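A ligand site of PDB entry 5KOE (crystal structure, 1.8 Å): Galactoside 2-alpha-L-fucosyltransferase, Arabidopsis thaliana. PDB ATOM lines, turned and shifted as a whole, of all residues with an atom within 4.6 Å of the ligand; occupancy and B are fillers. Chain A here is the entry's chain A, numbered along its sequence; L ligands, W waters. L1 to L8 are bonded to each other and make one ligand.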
ATOM      1  N   SER A  98      19.371 -32.482  18.039  1.00  0.00           N
ATOM      2  CA  SER A  98      19.232 -31.088  17.743  1.00  0.00           C
ATOM      3  C   SER A  98      17.985 -30.467  18.359  1.00  0.00           C
ATOM      4  O   SER A  98      17.286 -31.135  19.147  1.00  0.00           O
ATOM      5  CB  SER A  98      19.262 -30.891  16.166  1.00  0.00           C
ATOM      6  OG  SER A  98      19.521 -29.555  15.872  1.00  0.00           O
ATOM      7  N   ASN A 102      14.030 -28.578  14.436  1.00  0.00           N
ATOM      8  CA  ASN A 102      14.793 -29.516  13.568  1.00  0.00           C
ATOM      9  C   ASN A 102      14.232 -30.922  13.773  1.00  0.00           C
ATOM     10  O   ASN A 102      14.039 -31.673  12.832  1.00  0.00           O
ATOM     11  CB  ASN A 102      16.283 -29.520  13.940  1.00  0.00           C
ATOM     12  CG  ASN A 102      17.010 -28.283  13.468  1.00  0.00           C
ATOM     13  OD1 ASN A 102      16.530 -27.529  12.613  1.00  0.00           O
ATOM     14  ND2 ASN A 102      18.217 -28.103  13.954  1.00  0.00           N
ATOM     15  N   HIS A 189      23.899 -32.066   8.967  1.00  0.00           N
ATOM     16  CA  HIS A 189      24.239 -31.022   8.020  1.00  0.00           C
ATOM     17  C   HIS A 189      25.738 -31.075   7.578  1.00  0.00           C
ATOM     18  O   HIS A 189      26.064 -30.476   6.535  1.00  0.00           O
ATOM     19  CB  HIS A 189      24.008 -29.610   8.623  1.00  0.00           C
ATOM     20  CG  HIS A 189      24.861 -29.326   9.819  1.00  0.00           C
ATOM     21  ND1 HIS A 189      24.471 -29.621  11.092  1.00  0.00           N
ATOM     22  CD2 HIS A 189      26.018 -28.648   9.953  1.00  0.00           C
ATOM     23  CE1 HIS A 189      25.420 -29.344  11.950  1.00  0.00           C
ATOM     24  NE2 HIS A 189      26.382 -28.742  11.281  1.00  0.00           N
ATOM     25  N   TYR A 191      27.539 -33.629   6.701  1.00  0.00           N
ATOM     26  CA  TYR A 191      27.797 -34.896   6.015  1.00  0.00           C
ATOM     27  C   TYR A 191      28.589 -34.639   4.756  1.00  0.00           C
ATOM     28  O   TYR A 191      28.605 -33.466   4.239  1.00  0.00           O
ATOM     29  CB  TYR A 191      26.483 -35.675   5.748  1.00  0.00           C
ATOM     30  CG  TYR A 191      25.453 -35.136   4.804  1.00  0.00           C
ATOM     31  CD1 TYR A 191      25.305 -33.773   4.526  1.00  0.00           C
ATOM     32  CD2 TYR A 191      24.465 -36.003   4.342  1.00  0.00           C
ATOM     33  CE1 TYR A 191      24.248 -33.288   3.759  1.00  0.00           C
ATOM     34  CE2 TYR A 191      23.375 -35.542   3.659  1.00  0.00           C
ATOM     35  CZ  TYR A 191      23.322 -34.187   3.267  1.00  0.00           C
ATOM     36  OH  TYR A 191      22.308 -33.746   2.517  1.00  0.00           O
ATOM     37  N   LYS A 196      26.131 -38.675   1.411  1.00  0.00           N
ATOM     38  CA  LYS A 196      25.117 -38.154   0.449  1.00  0.00           C
ATOM     39  C   LYS A 196      24.639 -39.165  -0.644  1.00  0.00           C
ATOM     40  O   LYS A 196      23.612 -38.978  -1.310  1.00  0.00           O
ATOM     41  CB  LYS A 196      25.590 -36.860  -0.131  1.00  0.00           C
ATOM     42  CG  LYS A 196      25.588 -35.599   0.777  1.00  0.00           C
ATOM     43  CD  LYS A 196      26.401 -34.482   0.103  1.00  0.00           C
ATOM     44  CE  LYS A 196      26.450 -33.256   0.979  1.00  0.00           C
ATOM     45  NZ  LYS A 196      27.319 -32.252   0.252  1.00  0.00           N
ATOM     46  N   ASP A 218      19.483 -33.360  11.258  1.00  0.00           N
ATOM     47  CA  ASP A 218      18.881 -32.159  11.695  1.00  0.00           C
ATOM     48  C   ASP A 218      18.244 -31.406  10.475  1.00  0.00           C
ATOM     49  O   ASP A 218      17.845 -30.218  10.664  1.00  0.00           O
ATOM     50  CB  ASP A 218      19.887 -31.300  12.385  1.00  0.00           C
ATOM     51  CG  ASP A 218      21.189 -31.076  11.546  1.00  0.00           C
ATOM     52  OD1 ASP A 218      21.337 -31.550  10.351  1.00  0.00           O
ATOM     53  OD2 ASP A 218      22.065 -30.355  12.045  1.00  0.00           O
ATOM     54  N   ASN A 219      18.010 -32.092   9.334  1.00  0.00           N
ATOM     55  CA  ASN A 219      17.400 -31.416   8.188  1.00  0.00           C
ATOM     56  C   ASN A 219      16.024 -32.002   7.792  1.00  0.00           C
ATOM     57  O   ASN A 219      15.745 -33.209   7.993  1.00  0.00           O
ATOM     58  CB  ASN A 219      18.323 -31.554   7.004  1.00  0.00           C
ATOM     59  CG  ASN A 219      19.380 -30.446   6.937  1.00  0.00           C
ATOM     60  OD1 ASN A 219      19.441 -29.711   5.949  1.00  0.00           O
ATOM     61  ND2 ASN A 219      20.229 -30.313   7.935  1.00  0.00           N
ATOM     62  N   PHE A 286      19.184 -14.508  14.342  1.00  0.00           N
ATOM     63  CA  PHE A 286      20.394 -15.326  14.488  1.00  0.00           C
ATOM     64  C   PHE A 286      21.556 -14.374  14.731  1.00  0.00           C
ATOM     65  O   PHE A 286      22.166 -13.879  13.779  1.00  0.00           O
ATOM     66  CB  PHE A 286      20.630 -16.242  13.247  1.00  0.00           C
ATOM     67  CG  PHE A 286      19.569 -17.321  13.050  1.00  0.00           C
ATOM     68  CD1 PHE A 286      19.642 -18.492  13.746  1.00  0.00           C
ATOM     69  CD2 PHE A 286      18.470 -17.113  12.207  1.00  0.00           C
ATOM     70  CE1 PHE A 286      18.632 -19.463  13.633  1.00  0.00           C
ATOM     71  CE2 PHE A 286      17.469 -18.093  12.054  1.00  0.00           C
ATOM     72  CZ  PHE A 286      17.548 -19.273  12.782  1.00  0.00           C
ATOM     73  N   ASP A 287      21.820 -14.078  15.989  1.00  0.00           N
ATOM     74  CA  ASP A 287      22.877 -13.151  16.365  1.00  0.00           C
ATOM     75  C   ASP A 287      23.409 -13.475  17.729  1.00  0.00           C
ATOM     76  O   ASP A 287      22.641 -13.718  18.637  1.00  0.00           O
ATOM     77  CB  ASP A 287      22.376 -11.714  16.379  1.00  0.00           C
ATOM     78  CG  ASP A 287      23.548 -10.651  16.280  1.00  0.00           C
ATOM     79  OD1 ASP A 287      24.367 -10.462  17.233  1.00  0.00           O
ATOM     80  OD2 ASP A 287      23.591  -9.948  15.248  1.00  0.00           O
ATOM     81  N   GLU A 288      24.716 -13.362  17.846  1.00  0.00           N
ATOM     82  CA  GLU A 288      25.476 -13.403  19.107  1.00  0.00           C
ATOM     83  C   GLU A 288      24.981 -12.471  20.239  1.00  0.00           C
ATOM     84  O   GLU A 288      24.746 -12.926  21.354  1.00  0.00           O
ATOM     85  CB  GLU A 288      26.959 -13.064  18.795  1.00  0.00           C
ATOM     86  N   TRP A 399      15.354 -18.835   7.586  1.00  0.00           N
ATOM     87  CA  TRP A 399      16.123 -19.934   8.140  1.00  0.00           C
ATOM     88  C   TRP A 399      15.499 -20.643   9.368  1.00  0.00           C
ATOM     89  O   TRP A 399      16.148 -21.566   9.833  1.00  0.00           O
ATOM     90  CB  TRP A 399      17.576 -19.529   8.526  1.00  0.00           C
ATOM     91  CG  TRP A 399      18.479 -19.035   7.385  1.00  0.00           C
ATOM     92  CD1 TRP A 399      18.137 -18.283   6.292  1.00  0.00           C
ATOM     93  CD2 TRP A 399      19.872 -19.345   7.243  1.00  0.00           C
ATOM     94  NE1 TRP A 399      19.267 -17.951   5.577  1.00  0.00           N
ATOM     95  CE2 TRP A 399      20.319 -18.699   6.071  1.00  0.00           C
ATOM     96  CE3 TRP A 399      20.771 -20.144   7.982  1.00  0.00           C
ATOM     97  CZ2 TRP A 399      21.632 -18.807   5.613  1.00  0.00           C
ATOM     98  CZ3 TRP A 399      22.128 -20.225   7.543  1.00  0.00           C
ATOM     99  CH2 TRP A 399      22.541 -19.514   6.397  1.00  0.00           C
ATOM    100  N   THR A 401      13.513 -23.057  11.488  1.00  0.00           N
ATOM    101  CA  THR A 401      12.730 -24.300  11.400  1.00  0.00           C
ATOM    102  C   THR A 401      11.538 -24.227  12.318  1.00  0.00           C
ATOM    103  O   THR A 401      10.516 -24.837  12.018  1.00  0.00           O
ATOM    104  CB  THR A 401      13.577 -25.520  11.732  1.00  0.00           C
ATOM    105  OG1 THR A 401      14.232 -25.292  12.981  1.00  0.00           O
ATOM    106  CG2 THR A 401      14.586 -25.738  10.583  1.00  0.00           C
ATOM    107  N   ARG A 419      16.733 -12.699   5.896  1.00  0.00           N
ATOM    108  CA  ARG A 419      17.812 -12.657   6.823  1.00  0.00           C
ATOM    109  C   ARG A 419      18.647 -11.396   6.686  1.00  0.00           C
ATOM    110  O   ARG A 419      19.261 -11.183   5.637  1.00  0.00           O
ATOM    111  CB  ARG A 419      18.695 -13.922   6.682  1.00  0.00           C
ATOM    112  CG  ARG A 419      19.847 -13.941   7.702  1.00  0.00           C
ATOM    113  CD  ARG A 419      20.504 -15.296   7.730  1.00  0.00           C
ATOM    114  NE  ARG A 419      21.687 -15.332   8.603  1.00  0.00           N
ATOM    115  CZ  ARG A 419      22.071 -16.371   9.351  1.00  0.00           C
ATOM    116  NH1 ARG A 419      21.331 -17.468   9.418  1.00  0.00           N
ATOM    117  NH2 ARG A 419      23.165 -16.266  10.110  1.00  0.00           N
ATOM    118  N   GLU A 421      21.848  -8.924   6.864  1.00  0.00           N
ATOM    119  CA  GLU A 421      23.308  -8.921   6.956  1.00  0.00           C
ATOM    120  C   GLU A 421      23.692  -7.549   7.541  1.00  0.00           C
ATOM    121  O   GLU A 421      23.043  -6.556   7.241  1.00  0.00           O
ATOM    122  CB  GLU A 421      24.002  -9.161   5.594  1.00  0.00           C
ATOM    123  CG  GLU A 421      23.468 -10.331   4.690  1.00  0.00           C
ATOM    124  CD  GLU A 421      23.961 -11.769   5.041  1.00  0.00           C
ATOM    125  OE1 GLU A 421      23.122 -12.647   5.420  1.00  0.00           O
ATOM    126  OE2 GLU A 421      25.191 -12.060   4.878  1.00  0.00           O
ATOM    127  N   HIS A 441      17.824 -27.433   4.186  1.00  0.00           N
ATOM    128  CA  HIS A 441      18.947 -26.517   4.279  1.00  0.00           C
ATOM    129  C   HIS A 441      20.243 -27.000   3.696  1.00  0.00           C
ATOM    130  O   HIS A 441      20.986 -26.205   3.073  1.00  0.00           O
ATOM    131  CB  HIS A 441      19.179 -26.083   5.718  1.00  0.00           C
ATOM    132  CG  HIS A 441      18.102 -25.208   6.230  1.00  0.00           C
ATOM    133  ND1 HIS A 441      18.189 -24.552   7.413  1.00  0.00           N
ATOM    134  CD2 HIS A 441      17.033 -24.653   5.585  1.00  0.00           C
ATOM    135  CE1 HIS A 441      17.084 -23.861   7.610  1.00  0.00           C
ATOM    136  NE2 HIS A 441      16.423 -23.807   6.469  1.00  0.00           N
ATOM    137  N   SER A 442      20.532 -28.293   3.778  1.00  0.00           N
ATOM    138  CA  SER A 442      21.832 -28.847   3.327  1.00  0.00           C
ATOM    139  C   SER A 442      21.674 -30.027   2.341  1.00  0.00           C
ATOM    140  O   SER A 442      22.065 -31.206   2.618  1.00  0.00           O
ATOM    141  CB  SER A 442      22.720 -29.204   4.564  1.00  0.00           C
ATOM    142  OG  SER A 442      22.903 -28.000   5.403  1.00  0.00           O
ATOM    143  N   PRO A 443      21.093 -29.781   1.128  1.00  0.00           N
ATOM    144  CA  PRO A 443      20.880 -30.868   0.154  1.00  0.00           C
ATOM    145  C   PRO A 443      22.115 -31.298  -0.581  1.00  0.00           C
ATOM    146  O   PRO A 443      23.074 -30.556  -0.636  1.00  0.00           O
ATOM    147  CB  PRO A 443      19.931 -30.267  -0.884  1.00  0.00           C
ATOM    148  CG  PRO A 443      20.123 -28.799  -0.760  1.00  0.00           C
ATOM    149  CD  PRO A 443      20.669 -28.485   0.623  1.00  0.00           C
ATOM    150  N   PRO A 444      22.141 -32.515  -1.106  1.00  0.00           N
ATOM    151  CA  PRO A 444      23.191 -32.920  -2.018  1.00  0.00           C
ATOM    152  C   PRO A 444      22.997 -32.188  -3.390  1.00  0.00           C
ATOM    153  O   PRO A 444      21.848 -31.876  -3.822  1.00  0.00           O
ATOM    154  CB  PRO A 444      22.956 -34.383  -2.192  1.00  0.00           C
ATOM    155  CG  PRO A 444      21.510 -34.576  -2.011  1.00  0.00           C
ATOM    156  CD  PRO A 444      21.050 -33.518  -1.042  1.00  0.00           C
ATOM    157  N   PHE A 445      24.133 -32.057  -4.048  1.00  0.00           N
ATOM    158  CA  PHE A 445      24.224 -31.469  -5.359  1.00  0.00           C
ATOM    159  C   PHE A 445      24.930 -32.454  -6.270  1.00  0.00           C
ATOM    160  O   PHE A 445      25.931 -32.109  -6.805  1.00  0.00           O
ATOM    161  CB  PHE A 445      24.977 -30.169  -5.205  1.00  0.00           C
ATOM    162  CG  PHE A 445      24.131 -29.061  -4.613  1.00  0.00           C
ATOM    163  CD1 PHE A 445      23.383 -28.272  -5.436  1.00  0.00           C
ATOM    164  CD2 PHE A 445      24.098 -28.784  -3.238  1.00  0.00           C
ATOM    165  CE1 PHE A 445      22.639 -27.201  -4.917  1.00  0.00           C
ATOM    166  CE2 PHE A 445      23.360 -27.732  -2.739  1.00  0.00           C
ATOM    167  CZ  PHE A 445      22.563 -26.980  -3.552  1.00  0.00           C
ATOM    168  N   TRP A 471      20.709 -21.730  -1.313  1.00  0.00           N
ATOM    169  CA  TRP A 471      21.073 -23.073  -1.696  1.00  0.00           C
ATOM    170  C   TRP A 471      20.177 -24.272  -1.224  1.00  0.00           C
ATOM    171  O   TRP A 471      20.421 -25.399  -1.665  1.00  0.00           O
ATOM    172  CB  TRP A 471      22.524 -23.345  -1.257  1.00  0.00           C
ATOM    173  CG  TRP A 471      22.671 -23.195   0.179  1.00  0.00           C
ATOM    174  CD1 TRP A 471      22.435 -24.165   1.118  1.00  0.00           C
ATOM    175  CD2 TRP A 471      23.133 -22.035   0.876  1.00  0.00           C
ATOM    176  NE1 TRP A 471      22.630 -23.636   2.359  1.00  0.00           N
ATOM    177  CE2 TRP A 471      23.121 -22.350   2.230  1.00  0.00           C
ATOM    178  CE3 TRP A 471      23.640 -20.777   0.464  1.00  0.00           C
ATOM    179  CZ2 TRP A 471      23.506 -21.442   3.231  1.00  0.00           C
ATOM    180  CZ3 TRP A 471      24.040 -19.867   1.448  1.00  0.00           C
ATOM    181  CH2 TRP A 471      23.997 -20.206   2.816  1.00  0.00           C
HETATM  182  C1  LIG L   1      25.557 -21.149  17.886  1.00  0.00           C
HETATM  183  C2  LIG L   1      25.840 -21.019  16.375  1.00  0.00           C
HETATM  184  C3  LIG L   1      24.804 -20.148  15.601  1.00  0.00           C
HETATM  185  C4  LIG L   1      24.328 -18.961  16.407  1.00  0.00           C
HETATM  186  C5  LIG L   1      23.126 -18.333  15.709  1.00  0.00           C
HETATM  187  C6  LIG L   1      25.162 -19.789  18.416  1.00  0.00           C
HETATM  188  O1  LIG L   1      24.918 -19.833  19.825  1.00  0.00           O
HETATM  189  O2  LIG L   1      26.755 -21.595  18.588  1.00  0.00           O
HETATM  190  O3  LIG L   1      25.849 -22.339  15.793  1.00  0.00           O
HETATM  191  O4  LIG L   1      25.467 -19.595  14.438  1.00  0.00           O
HETATM  192  O5  LIG L   1      23.967 -19.393  17.733  1.00  0.00           O
HETATM  193  O6  LIG L   1      22.710 -17.228  16.524  1.00  0.00           O
HETATM  194  C1  LG2 L   2      25.418 -18.964  12.063  1.00  0.00           C
HETATM  195  C2  LG2 L   2      25.163 -19.492  10.647  1.00  0.00           C
HETATM  196  C3  LG2 L   2      25.485 -20.972  10.477  1.00  0.00           C
HETATM  197  C4  LG2 L   2      24.925 -21.794  11.612  1.00  0.00           C
HETATM  198  C5  LG2 L   2      25.257 -23.273  11.382  1.00  0.00           C
HETATM  199  C6  LG2 L   2      24.956 -19.985  13.140  1.00  0.00           C
HETATM  200  O1  LG2 L   2      24.644 -17.756  12.212  1.00  0.00           O
HETATM  201  O2  LG2 L   2      25.956 -18.750   9.696  1.00  0.00           O
HETATM  202  O3  LG2 L   2      24.819 -21.453   9.250  1.00  0.00           O
HETATM  203  O4  LG2 L   2      25.477 -21.307  12.838  1.00  0.00           O
HETATM  204  O5  LG2 L   2      24.865 -23.961  12.563  1.00  0.00           O
HETATM  205  C1  LG3 L   3      25.104 -22.897   7.312  1.00  0.00           C
HETATM  206  C2  LG3 L   3      26.129 -23.295   6.314  1.00  0.00           C
HETATM  207  C3  LG3 L   3      26.577 -22.065   5.534  1.00  0.00           C
HETATM  208  C4  LG3 L   3      27.006 -20.939   6.428  1.00  0.00           C
HETATM  209  C5  LG3 L   3      27.088 -19.717   5.528  1.00  0.00           C
HETATM  210  C6  LG3 L   3      25.746 -21.864   8.233  1.00  0.00           C
HETATM  211  O1  LG3 L   3      24.733 -24.086   8.036  1.00  0.00           O
HETATM  212  O2  LG3 L   3      25.576 -24.306   5.400  1.00  0.00           O
HETATM  213  O3  LG3 L   3      27.756 -22.432   4.780  1.00  0.00           O
HETATM  214  O4  LG3 L   3      26.042 -20.664   7.464  1.00  0.00           O
HETATM  215  O5  LG3 L   3      27.362 -18.612   6.391  1.00  0.00           O
HETATM  216  C1  LG4 L   4      24.851 -25.405  12.300  1.00  0.00           C
HETATM  217  C2  LG4 L   4      23.843 -26.135  13.190  1.00  0.00           C
HETATM  218  C3  LG4 L   4      24.258 -25.949  14.647  1.00  0.00           C
HETATM  219  C4  LG4 L   4      25.626 -26.464  14.882  1.00  0.00           C
HETATM  220  C5  LG4 L   4      26.566 -25.804  13.966  1.00  0.00           C
HETATM  221  O1  LG4 L   4      22.506 -25.566  13.076  1.00  0.00           O
HETATM  222  O2  LG4 L   4      23.299 -26.612  15.499  1.00  0.00           O
HETATM  223  O3  LG4 L   4      25.947 -26.029  16.175  1.00  0.00           O
HETATM  224  O4  LG4 L   4      26.161 -25.958  12.542  1.00  0.00           O
HETATM  225  C1  LG5 L   5      28.916 -22.257   2.733  1.00  0.00           C
HETATM  226  C2  LG5 L   5      28.786 -22.364   1.179  1.00  0.00           C
HETATM  227  C3  LG5 L   5      27.914 -23.569   0.831  1.00  0.00           C
HETATM  228  C4  LG5 L   5      26.605 -23.501   1.614  1.00  0.00           C
HETATM  229  C5  LG5 L   5      25.741 -24.695   1.268  1.00  0.00           C
HETATM  230  C6  LG5 L   5      27.537 -22.339   3.397  1.00  0.00           C
HETATM  231  O1  LG5 L   5      29.501 -20.989   3.140  1.00  0.00           O
HETATM  232  O2  LG5 L   5      30.116 -22.560   0.589  1.00  0.00           O
HETATM  233  O3  LG5 L   5      27.577 -23.542  -0.535  1.00  0.00           O
HETATM  234  O4  LG5 L   5      26.831 -23.522   3.020  1.00  0.00           O
HETATM  235  O5  LG5 L   5      26.486 -25.887   1.531  1.00  0.00           O
HETATM  236  C1  LG6 L   6      27.288 -17.350   5.687  1.00  0.00           C
HETATM  237  C2  LG6 L   6      28.018 -16.305   6.513  1.00  0.00           C
HETATM  238  C3  LG6 L   6      27.175 -16.095   7.764  1.00  0.00           C
HETATM  239  C4  LG6 L   6      25.936 -15.271   7.338  1.00  0.00           C
HETATM  240  C5  LG6 L   6      25.452 -15.637   5.884  1.00  0.00           C
HETATM  241  O1  LG6 L   6      29.333 -16.736   6.861  1.00  0.00           O
HETATM  242  O2  LG6 L   6      27.938 -15.430   8.790  1.00  0.00           O
HETATM  243  O3  LG6 L   6      24.884 -15.502   8.274  1.00  0.00           O
HETATM  244  O4  LG6 L   6      25.842 -16.987   5.536  1.00  0.00           O
HETATM  245  C1  LG7 L   7      21.616 -26.349  12.206  1.00  0.00           C
HETATM  246  C2  LG7 L   7      20.241 -25.684  12.168  1.00  0.00           C
HETATM  247  C3  LG7 L   7      19.325 -26.471  11.171  1.00  0.00           C
HETATM  248  C4  LG7 L   7      19.949 -26.418   9.753  1.00  0.00           C
HETATM  249  C5  LG7 L   7      21.333 -27.031   9.814  1.00  0.00           C
HETATM  250  C6  LG7 L   7      22.040 -26.805   8.488  1.00  0.00           C
HETATM  251  O1  LG7 L   7      19.680 -25.729  13.466  1.00  0.00           O
HETATM  252  O2  LG7 L   7      18.005 -25.920  11.140  1.00  0.00           O
HETATM  253  O3  LG7 L   7      20.038 -25.064   9.316  1.00  0.00           O
HETATM  254  O4  LG7 L   7      22.188 -26.383  10.796  1.00  0.00           O
HETATM  255  O5  LG7 L   7      21.534 -27.870   7.683  1.00  0.00           O
HETATM  256  C1  LG8 L   8      25.812 -26.774   2.552  1.00  0.00           C
HETATM  257  C2  LG8 L   8      26.653 -28.004   2.872  1.00  0.00           C
HETATM  258  C3  LG8 L   8      26.810 -28.860   1.627  1.00  0.00           C
HETATM  259  C4  LG8 L   8      25.429 -29.215   1.043  1.00  0.00           C
HETATM  260  C5  LG8 L   8      24.604 -27.932   0.819  1.00  0.00           C
HETATM  261  O1  LG8 L   8      27.980 -27.607   3.284  1.00  0.00           O
HETATM  262  O2  LG8 L   8      27.532 -30.066   1.966  1.00  0.00           O
HETATM  263  O3  LG8 L   8      25.643 -29.922  -0.228  1.00  0.00           O
HETATM  264  O4  LG8 L   8      24.570 -27.231   2.062  1.00  0.00           O
HETATM  265  O   HOH W   1      27.995 -19.019   2.296  1.00  0.00           O
HETATM  266  O   HOH W   2      21.435 -23.434   7.005  1.00  0.00           O
HETATM  267  O   HOH W   3      29.884 -26.909   0.902  1.00  0.00           O
HETATM  268  O   HOH W   4      16.941 -27.906   9.118  1.00  0.00           O
HETATM  269  O   HOH W   5      22.158 -29.416  14.662  1.00  0.00           O
HETATM  270  O   HOH W   6      23.546 -12.633   7.964  1.00  0.00           O
HETATM  271  O   HOH W   7      30.663 -29.499   1.950  1.00  0.00           O
HETATM  272  O   HOH W   8      17.204 -24.536  14.577  1.00  0.00           O
HETATM  273  O   HOH W   9      21.690 -19.056  11.542  1.00  0.00           O
HETATM  274  O   HOH W  10      22.291 -23.252   9.379  1.00  0.00           O
HETATM  275  O   HOH W  11      18.275 -22.767  10.926  1.00  0.00           O
HETATM  276  O   HOH W  12      22.178 -22.563  13.508  1.00  0.00           O
HETATM  277  O   HOH W  13      27.936 -30.912   4.566  1.00  0.00           O
HETATM  278  O   HOH W  14      23.022 -24.766   5.111  1.00  0.00           O
HETATM  279  O   HOH W  15      25.551 -27.638   6.012  1.00  0.00           O
HETATM  280  O   HOH W  16      31.511 -24.463   1.648  1.00  0.00           O
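Water W14 lies within hydrogen-bond range of an oxygen (O2) of LG3 L3 (2.6 Å), the indole nitrogen of Trp 471 (3.0 Å), the backbone carbonyl oxygen of His 441 (3.2 Å) and the side-chain hydroxyl of Ser 442 (3.2 Å). Water W13 lies within hydrogen-bond range of the backbone carbonyl oxygen of Tyr 191, the backbone carbonyl oxygen of His 189 and an oxygen (O2) of LG8 L8. Water W5 lies within hydrogen-bond range of OD2 of Asp 218, OG of Ser 98 and O2 of LG4 L4. Water W2 bridges an oxygen (O3) of LG7 L7 (3.2 Å) and a ring nitrogen (ND1) of His 441 (3.5 Å). Water W6 lies within hydrogen-bond range of OE1 of Glu 421 (2.6 Å), O3 of LG6 L6 (3.2 Å) and NE of Arg 419 (3.3 Å). Water W15 lies within hydrogen-bond range of the side-chain hydroxyl (OG) of Ser 442 (2.7 Å), the backbone carbonyl oxygen (O) of His 189 (2.9 Å) and an oxygen (O2) of LG3 L3 (3.4 Å).
OG1 of Thr 401 lies within hydrogen-bond range of OD1 of Asn 102 (3.2 Å). ND2 of Asn 102 is in hydrogen-bond range of OG of Ser 98 (2.7 Å). OD1 of Asn 219 is in hydrogen-bond range of N of Ser 442 (2.8 Å). The side-chain hydroxyl (OH) of Tyr 191 is in hydrogen-bond range of the backbone carbonyl oxygen (O) of Ser 442. The side-chain amide oxygen (OD1) of Asn 219 is in hydrogen-bond range of the backbone NH (N) of His 441. The backbone carbonyl oxygen (O) of His 441 lies within hydrogen-bond range of the indole nitrogen (NE1) of Trp 471 (3.1 Å). The side-chain amide nitrogen (ND2) of Asn 219 sits at hydrogen-bond distance from the side-chain carboxylate (OD1) of Asp 218 (2.9 Å). A ring nitrogen (ND1) of His 189 is in hydrogen-bond range of the side-chain carboxylate of Asp 218 (2.7 Å).
An oxygen (O3) of LG6 L6 sits at hydrogen-bond distance from the guanidinium group (NH2) of Arg 419 (2.6 Å). OD1 of Asn 102 is in hydrogen-bond range of O2 of LG7 L7, at 2.6 Å. OG of Ser 442 sits at hydrogen-bond distance from O5 of LG7 L7 (2.7 Å). O3 of LG8 L8 sits at hydrogen-bond distance from O of Pro 443 (2.7 Å). ND1 of His 441 sits at hydrogen-bond distance from O3 of LG7 L7, 2.7 Å away. The side-chain amide nitrogen (ND2) of Asn 219 lies within hydrogen-bond range of an oxygen (O5) of LG7 L7 (2.8 Å). The side-chain amino group of Lys 196 sits at hydrogen-bond distance from an oxygen (O2) of LG8 L8 (2.8 Å). NE2 of His 189 sits at hydrogen-bond distance from O4 of LG4 L4 (3.1 Å). O6 of LIG L1 is in hydrogen-bond range of N of Asp 287 (3.3 Å).
Merely in contact with the ligand: Phe 286, Trp 399, Thr 401, Glu 421, Phe 445 and Trp 471. Hydrophobic or aromatic side chains that line the ligand: His 189, Trp 399, His 441, Pro 443, Phe 445 and Trp 471. Within 4 Å of the ligand: Asn 102, His 189, Lys 196, Asn 219, Phe 286, Asp 287, Trp 399, Thr 401, Arg 419, Glu 421, His 441, Ser 442, Pro 443, Phe 445 and Trp 471.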
